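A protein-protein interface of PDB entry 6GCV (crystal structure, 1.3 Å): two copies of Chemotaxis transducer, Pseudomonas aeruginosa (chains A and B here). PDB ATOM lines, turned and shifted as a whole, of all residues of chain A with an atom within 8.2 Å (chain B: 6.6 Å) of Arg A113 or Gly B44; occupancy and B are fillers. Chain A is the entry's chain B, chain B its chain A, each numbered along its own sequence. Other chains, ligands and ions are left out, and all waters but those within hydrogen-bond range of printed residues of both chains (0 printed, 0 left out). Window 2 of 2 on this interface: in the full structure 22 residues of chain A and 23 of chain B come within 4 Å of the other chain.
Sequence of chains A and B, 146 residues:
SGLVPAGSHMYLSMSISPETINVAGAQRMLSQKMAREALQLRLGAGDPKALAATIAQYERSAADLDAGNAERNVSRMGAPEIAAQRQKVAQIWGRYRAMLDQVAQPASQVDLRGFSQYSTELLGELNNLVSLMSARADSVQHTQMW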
ATOM      1  N   LEU A  43       7.538  34.469  -2.818  1.00  0.00           N
ATOM      2  CA  LEU A  43       8.833  34.720  -2.179  1.00  0.00           C
ATOM      3  C   LEU A  43       9.841  35.436  -3.051  1.00  0.00           C
ATOM      4  O   LEU A  43      10.959  35.664  -2.610  1.00  0.00           O
ATOM      5  CB  LEU A  43       9.385  33.381  -1.670  1.00  0.00           C
ATOM      6  CG  LEU A  43       8.681  32.824  -0.414  1.00  0.00           C
ATOM      7  CD1 LEU A  43       8.888  31.327  -0.257  1.00  0.00           C
ATOM      8  CD2 LEU A  43       9.185  33.539   0.824  1.00  0.00           C
ATOM      9  N   VAL A 103      -1.883  34.211  -4.988  1.00  0.00           N
ATOM     10  CA  VAL A 103      -0.772  33.721  -4.200  1.00  0.00           C
ATOM     11  C   VAL A 103       0.555  34.198  -4.762  1.00  0.00           C
ATOM     12  O   VAL A 103       1.460  34.582  -4.052  1.00  0.00           O
ATOM     13  CB  VAL A 103      -0.814  32.188  -4.124  1.00  0.00           C
ATOM     14  CG1 VAL A 103       0.462  31.622  -3.497  1.00  0.00           C
ATOM     15  CG2 VAL A 103      -2.050  31.806  -3.349  1.00  0.00           C
ATOM     16  N   VAL A 110      -3.621  37.585   0.802  1.00  0.00           N
ATOM     17  CA  VAL A 110      -4.177  36.261   0.521  1.00  0.00           C
ATOM     18  C   VAL A 110      -4.158  35.470   1.816  1.00  0.00           C
ATOM     19  O   VAL A 110      -3.342  35.703   2.722  1.00  0.00           O
ATOM     20  CB  VAL A 110      -3.426  35.530  -0.608  1.00  0.00           C
ATOM     21  CG1 VAL A 110      -2.061  35.115  -0.135  1.00  0.00           C
ATOM     22  CG2 VAL A 110      -4.228  34.389  -1.205  1.00  0.00           C
ATOM     23  N   ASP A 111      -5.106  34.549   1.916  1.00  0.00           N
ATOM     24  CA  ASP A 111      -5.140  33.604   3.061  1.00  0.00           C
ATOM     25  C   ASP A 111      -4.477  32.295   2.661  1.00  0.00           C
ATOM     26  O   ASP A 111      -5.020  31.468   1.906  1.00  0.00           O
ATOM     27  CB  ASP A 111      -6.582  33.392   3.458  1.00  0.00           C
ATOM     28  CG  ASP A 111      -6.732  32.548   4.687  1.00  0.00           C
ATOM     29  OD1 ASP A 111      -5.884  31.743   4.968  1.00  0.00           O
ATOM     30  OD2 ASP A 111      -7.718  32.745   5.424  1.00  0.00           O
ATOM     31  N   LEU A 112      -3.225  32.158   3.097  1.00  0.00           N
ATOM     32  CA  LEU A 112      -2.421  31.042   2.670  1.00  0.00           C
ATOM     33  C   LEU A 112      -2.922  29.725   3.207  1.00  0.00           C
ATOM     34  O   LEU A 112      -2.792  28.705   2.541  1.00  0.00           O
ATOM     35  CB  LEU A 112      -0.948  31.245   3.026  1.00  0.00           C
ATOM     36  CG  LEU A 112      -0.229  32.349   2.278  1.00  0.00           C
ATOM     37  CD1 LEU A 112       1.157  32.534   2.852  1.00  0.00           C
ATOM     38  CD2 LEU A 112      -0.179  32.054   0.797  1.00  0.00           C
ATOM     39  N   ARG A 113      -3.511  29.703   4.397  1.00  0.00           N
ATOM     40  CA  ARG A 113      -4.095  28.485   4.899  1.00  0.00           C
ATOM     41  C   ARG A 113      -5.313  28.080   4.109  1.00  0.00           C
ATOM     42  O   ARG A 113      -5.491  26.892   3.853  1.00  0.00           O
ATOM     43  CB  ARG A 113      -4.402  28.580   6.390  1.00  0.00           C
ATOM     44  CG  ARG A 113      -3.141  28.654   7.236  1.00  0.00           C
ATOM     45  CD  ARG A 113      -3.472  28.842   8.689  1.00  0.00           C
ATOM     46  NE  ARG A 113      -2.264  29.056   9.479  1.00  0.00           N
ATOM     47  CZ  ARG A 113      -1.594  30.210   9.542  1.00  0.00           C
ATOM     48  NH1 ARG A 113      -2.022  31.288   8.918  1.00  0.00           N
ATOM     49  NH2 ARG A 113      -0.512  30.303  10.267  1.00  0.00           N
ATOM     50  N   GLY A 114      -6.105  29.039   3.665  1.00  0.00           N
ATOM     51  CA  GLY A 114      -7.206  28.741   2.759  1.00  0.00           C
ATOM     52  C   GLY A 114      -6.717  28.111   1.446  1.00  0.00           C
ATOM     53  O   GLY A 114      -7.297  27.153   0.923  1.00  0.00           O
ATOM     54  N   PHE A 115      -5.636  28.673   0.933  1.00  0.00           N
ATOM     55  CA  PHE A 115      -5.029  28.181  -0.293  1.00  0.00           C
ATOM     56  C   PHE A 115      -4.528  26.735  -0.138  1.00  0.00           C
ATOM     57  O   PHE A 115      -4.797  25.879  -0.983  1.00  0.00           O
ATOM     58  CB  PHE A 115      -3.877  29.090  -0.721  1.00  0.00           C
ATOM     59  CG  PHE A 115      -3.113  28.573  -1.893  1.00  0.00           C
ATOM     60  CD1 PHE A 115      -3.725  28.445  -3.126  1.00  0.00           C
ATOM     61  CD2 PHE A 115      -1.808  28.227  -1.767  1.00  0.00           C
ATOM     62  CE1 PHE A 115      -3.026  27.960  -4.210  1.00  0.00           C
ATOM     63  CE2 PHE A 115      -1.084  27.784  -2.863  1.00  0.00           C
ATOM     64  CZ  PHE A 115      -1.714  27.650  -4.061  1.00  0.00           C
ATOM     65  N   SER A 116      -3.799  26.464   0.942  1.00  0.00           N
ATOM     66  CA  SER A 116      -3.275  25.116   1.128  1.00  0.00           C
ATOM     67  C   SER A 116      -4.405  24.130   1.360  1.00  0.00           C
ATOM     68  O   SER A 116      -4.351  23.015   0.821  1.00  0.00           O
ATOM     69  CB  SER A 116      -2.215  25.053   2.217  1.00  0.00           C
ATOM     70  OG  SER A 116      -2.676  25.619   3.399  1.00  0.00           O
ATOM     71  N   GLN A 117      -5.447  24.520   2.083  1.00  0.00           N
ATOM     72  CA  GLN A 117      -6.591  23.635   2.210  1.00  0.00           C
ATOM     73  C   GLN A 117      -7.204  23.298   0.861  1.00  0.00           C
ATOM     74  O   GLN A 117      -7.553  22.147   0.600  1.00  0.00           O
ATOM     75  CB  GLN A 117      -7.633  24.249   3.138  1.00  0.00           C
ATOM     76  CG  GLN A 117      -7.216  24.315   4.614  1.00  0.00           C
ATOM     77  CD  GLN A 117      -8.083  25.252   5.449  1.00  0.00           C
ATOM     78  OE1 GLN A 117      -9.156  25.694   5.025  1.00  0.00           O
ATOM     79  NE2 GLN A 117      -7.609  25.563   6.648  1.00  0.00           N
ATOM     80  N   TYR A 118      -7.333  24.303   0.017  1.00  0.00           N
ATOM     81  CA  TYR A 118      -7.946  24.088  -1.281  1.00  0.00           C
ATOM     82  C   TYR A 118      -7.040  23.245  -2.192  1.00  0.00           C
ATOM     83  O   TYR A 118      -7.520  22.376  -2.944  1.00  0.00           O
ATOM     84  CB  TYR A 118      -8.344  25.441  -1.898  1.00  0.00           C
ATOM     85  CG  TYR A 118      -9.596  25.307  -2.755  1.00  0.00           C
ATOM     86  CD1 TYR A 118     -10.812  25.059  -2.176  1.00  0.00           C
ATOM     87  CD2 TYR A 118      -9.518  25.261  -4.134  1.00  0.00           C
ATOM     88  CE1 TYR A 118     -11.954  24.889  -2.916  1.00  0.00           C
ATOM     89  CE2 TYR A 118     -10.660  25.086  -4.914  1.00  0.00           C
ATOM     90  CZ  TYR A 118     -11.874  24.890  -4.297  1.00  0.00           C
ATOM     91  OH  TYR A 118     -12.995  24.708  -5.088  1.00  0.00           O
ATOM     92  N   SER A 119      -5.731  23.442  -2.086  1.00  0.00           N
ATOM     93  CA  SER A 119      -4.784  22.619  -2.836  1.00  0.00           C
ATOM     94  C   SER A 119      -4.923  21.151  -2.451  1.00  0.00           C
ATOM     95  O   SER A 119      -4.923  20.270  -3.305  1.00  0.00           O
ATOM     96  CB  SER A 119      -3.347  23.108  -2.566  1.00  0.00           C
ATOM     97  OG  SER A 119      -2.408  22.451  -3.402  1.00  0.00           O
ATOM     98  N   THR A 120      -5.037  20.901  -1.151  1.00  0.00           N
ATOM     99  CA  THR A 120      -5.215  19.543  -0.654  1.00  0.00           C
ATOM    100  C   THR A 120      -6.562  18.956  -1.072  1.00  0.00           C
ATOM    101  O   THR A 120      -6.668  17.773  -1.391  1.00  0.00           O
ATOM    102  CB  THR A 120      -4.939  19.505   0.839  1.00  0.00           C
ATOM    103  OG1 THR A 120      -3.542  19.811   1.020  1.00  0.00           O
ATOM    104  CG2 THR A 120      -5.247  18.161   1.439  1.00  0.00           C
ATOM    105  N   LEU B  39       7.714  25.809   1.707  1.00  0.00           N
ATOM    106  CA  LEU B  39       7.664  27.225   1.345  1.00  0.00           C
ATOM    107  C   LEU B  39       6.600  27.977   2.165  1.00  0.00           C
ATOM    108  O   LEU B  39       6.808  29.132   2.565  1.00  0.00           O
ATOM    109  CB  LEU B  39       7.392  27.384  -0.157  1.00  0.00           C
ATOM    110  CG  LEU B  39       8.546  26.883  -1.049  1.00  0.00           C
ATOM    111  CD1 LEU B  39       8.022  26.706  -2.465  1.00  0.00           C
ATOM    112  CD2 LEU B  39       9.718  27.810  -1.039  1.00  0.00           C
ATOM    113  N   GLN B  40       5.486  27.332   2.440  1.00  0.00           N
ATOM    114  CA  GLN B  40       4.470  27.951   3.273  1.00  0.00           C
ATOM    115  C   GLN B  40       4.962  28.184   4.732  1.00  0.00           C
ATOM    116  O   GLN B  40       4.673  29.203   5.349  1.00  0.00           O
ATOM    117  CB  GLN B  40       3.196  27.148   3.233  1.00  0.00           C
ATOM    118  CG  GLN B  40       2.021  27.890   3.839  1.00  0.00           C
ATOM    119  CD  GLN B  40       0.699  27.310   3.388  1.00  0.00           C
ATOM    120  OE1 GLN B  40       0.578  26.796   2.269  1.00  0.00           O
ATOM    121  NE2 GLN B  40      -0.301  27.381   4.248  1.00  0.00           N
ATOM    122  N   LEU B  41       5.712  27.216   5.236  1.00  0.00           N
ATOM    123  CA  LEU B  41       6.407  27.389   6.516  1.00  0.00           C
ATOM    124  C   LEU B  41       7.397  28.554   6.431  1.00  0.00           C
ATOM    125  O   LEU B  41       7.490  29.362   7.385  1.00  0.00           O
ATOM    126  CB  LEU B  41       7.118  26.093   6.936  1.00  0.00           C
ATOM    127  CG  LEU B  41       6.162  25.022   7.489  1.00  0.00           C
ATOM    128  CD1 LEU B  41       6.702  23.615   7.375  1.00  0.00           C
ATOM    129  CD2 LEU B  41       5.828  25.332   8.966  1.00  0.00           C
ATOM    130  N   ARG B  42       8.123  28.689   5.336  1.00  0.00           N
ATOM    131  CA  ARG B  42       9.038  29.819   5.237  1.00  0.00           C
ATOM    132  C   ARG B  42       8.328  31.161   5.342  1.00  0.00           C
ATOM    133  O   ARG B  42       8.861  32.122   5.904  1.00  0.00           O
ATOM    134  CB  ARG B  42       9.853  29.731   3.950  1.00  0.00           C
ATOM    135  CG  ARG B  42      11.033  30.676   3.958  1.00  0.00           C
ATOM    136  CD  ARG B  42      12.022  30.408   2.838  1.00  0.00           C
ATOM    137  NE  ARG B  42      13.223  31.181   2.975  1.00  0.00           N
ATOM    138  CZ  ARG B  42      14.179  30.946   3.880  1.00  0.00           C
ATOM    139  NH1 ARG B  42      14.141  29.848   4.608  1.00  0.00           N
ATOM    140  NH2 ARG B  42      15.194  31.781   3.975  1.00  0.00           N
ATOM    141  N   LEU B  43       7.107  31.196   4.841  1.00  0.00           N
ATOM    142  CA  LEU B  43       6.228  32.363   4.877  1.00  0.00           C
ATOM    143  C   LEU B  43       5.529  32.570   6.214  1.00  0.00           C
ATOM    144  O   LEU B  43       4.844  33.546   6.395  1.00  0.00           O
ATOM    145  CB  LEU B  43       5.192  32.267   3.740  1.00  0.00           C
ATOM    146  CG  LEU B  43       5.764  32.532   2.340  1.00  0.00           C
ATOM    147  CD1 LEU B  43       4.899  31.874   1.263  1.00  0.00           C
ATOM    148  CD2 LEU B  43       5.885  34.019   2.102  1.00  0.00           C
ATOM    149  N   GLY B  44       5.695  31.648   7.163  1.00  0.00           N
ATOM    150  CA  GLY B  44       5.095  31.805   8.504  1.00  0.00           C
ATOM    151  C   GLY B  44       3.645  31.418   8.582  1.00  0.00           C
ATOM    152  O   GLY B  44       2.979  31.766   9.578  1.00  0.00           O
ATOM    153  N   ALA B  45       3.137  30.698   7.567  1.00  0.00           N
ATOM    154  CA  ALA B  45       1.730  30.289   7.548  1.00  0.00           C
ATOM    155  C   ALA B  45       1.552  28.803   7.378  1.00  0.00           C
ATOM    156  O   ALA B  45       0.507  28.339   6.923  1.00  0.00           O
ATOM    157  CB  ALA B  45       0.965  31.044   6.469  1.00  0.00           C
ATOM    158  N   GLY B  46       2.559  28.040   7.813  1.00  0.00           N
ATOM    159  CA  GLY B  46       2.589  26.612   7.570  1.00  0.00           C
ATOM    160  C   GLY B  46       2.377  25.756   8.790  1.00  0.00           C
ATOM    161  O   GLY B  46       2.063  26.255   9.868  1.00  0.00           O
ATOM    162  N   PRO B 106      11.953  29.975   8.823  1.00  0.00           N
ATOM    163  CA  PRO B 106      11.889  31.329   8.279  1.00  0.00           C
ATOM    164  C   PRO B 106      13.156  32.132   8.339  1.00  0.00           C
ATOM    165  O   PRO B 106      13.367  32.991   7.496  1.00  0.00           O
ATOM    166  CB  PRO B 106      10.750  31.971   9.063  1.00  0.00           C
ATOM    167  CG  PRO B 106       9.865  30.809   9.402  1.00  0.00           C
ATOM    168  CD  PRO B 106      10.831  29.697   9.728  1.00  0.00           C
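O of Leu A112 sits at hydrogen-bond distance from NE2 of Gln B40, at 3.3 Å. The side-chain hydroxyl (OG) of Ser A116 lies within hydrogen-bond range of the side-chain amide nitrogen (NE2) of Gln B40 (3.1 Å).
OG1 of Thr A120 lies within hydrogen-bond range of O of Ser A116. OD1 of Asp A111 lies within hydrogen-bond range of N of Arg A113 (3.2 Å). The side-chain amide nitrogen (NE2) of Gln B40 is in hydrogen-bond range of the backbone carbonyl oxygen (O) of Ala B45 (3.0 Å). O of Arg A113 is in hydrogen-bond range of OG of Ser A116 (3.1 Å). OG of Ser A116 is in hydrogen-bond range of O of Leu A112 (3.2 Å). O of Gln B40 sits at hydrogen-bond distance from N of Gly B46, 3.4 Å away.
Leu B39 touches Leu A43 (CD2 to CD1, 3.7 Å). Leu B43 touches Leu A43. Ala B45 touches Leu A112 (CB to CD1, 3.9 Å). Arg A113 touches Gln B40. Arg A113 touches Gly B44 (NH2 to O, 3.8 Å). Arg A113 touches Ala B45.
Arg A113 touches just these residues of chain B: Gln B40, Gly B44 and Ala B45. Of chain A, only Arg A113 (3.8 Å) comes within 4 Å of Gly B44. Of chain A, only Leu A112 (3.9 Å) and Arg A113 (3.5 Å) come within 4 Å of Ala B45. Of the printed residues of chain A, Gln B40 touches Leu A112 (3.3 Å), Arg A113 (3.96 Å) and Ser A116 (3.1 Å). Of the printed residues of chain B, Leu A43 touches Leu B39 and Leu B43. Of the printed residues of chain A, Leu B39 touches Leu A43. The nearest residue of chain B that does not touch Arg A113 is Gly B46 (4.5 Å). The nearest residue of chain A that does not touch Gly B44 is Leu A112 (6.3 Å).
Printed residues of chain A that touch a printed residue of chain B: Leu A43, Leu A112, Arg A113 and Ser A116. Hydrophobic or aromatic side chains of chain A within 4 Å of the printed part of chain B: Leu A43 and Leu A112. Of the 9 printed residues of chain B, 5 touch a printed residue of chain A. Hydrophobic or aromatic side chains of chain B within 4 Å of the printed part of chain A: Leu B39, Leu B43 and Ala B45. Among the printed residues, no Asp or Glu carboxylate lies within 4 Å of a Lys or Arg side-chain nitrogen of the other chain.
Leu A43 touches its own counterpart, Leu B43. 1 position is printed for both chains.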
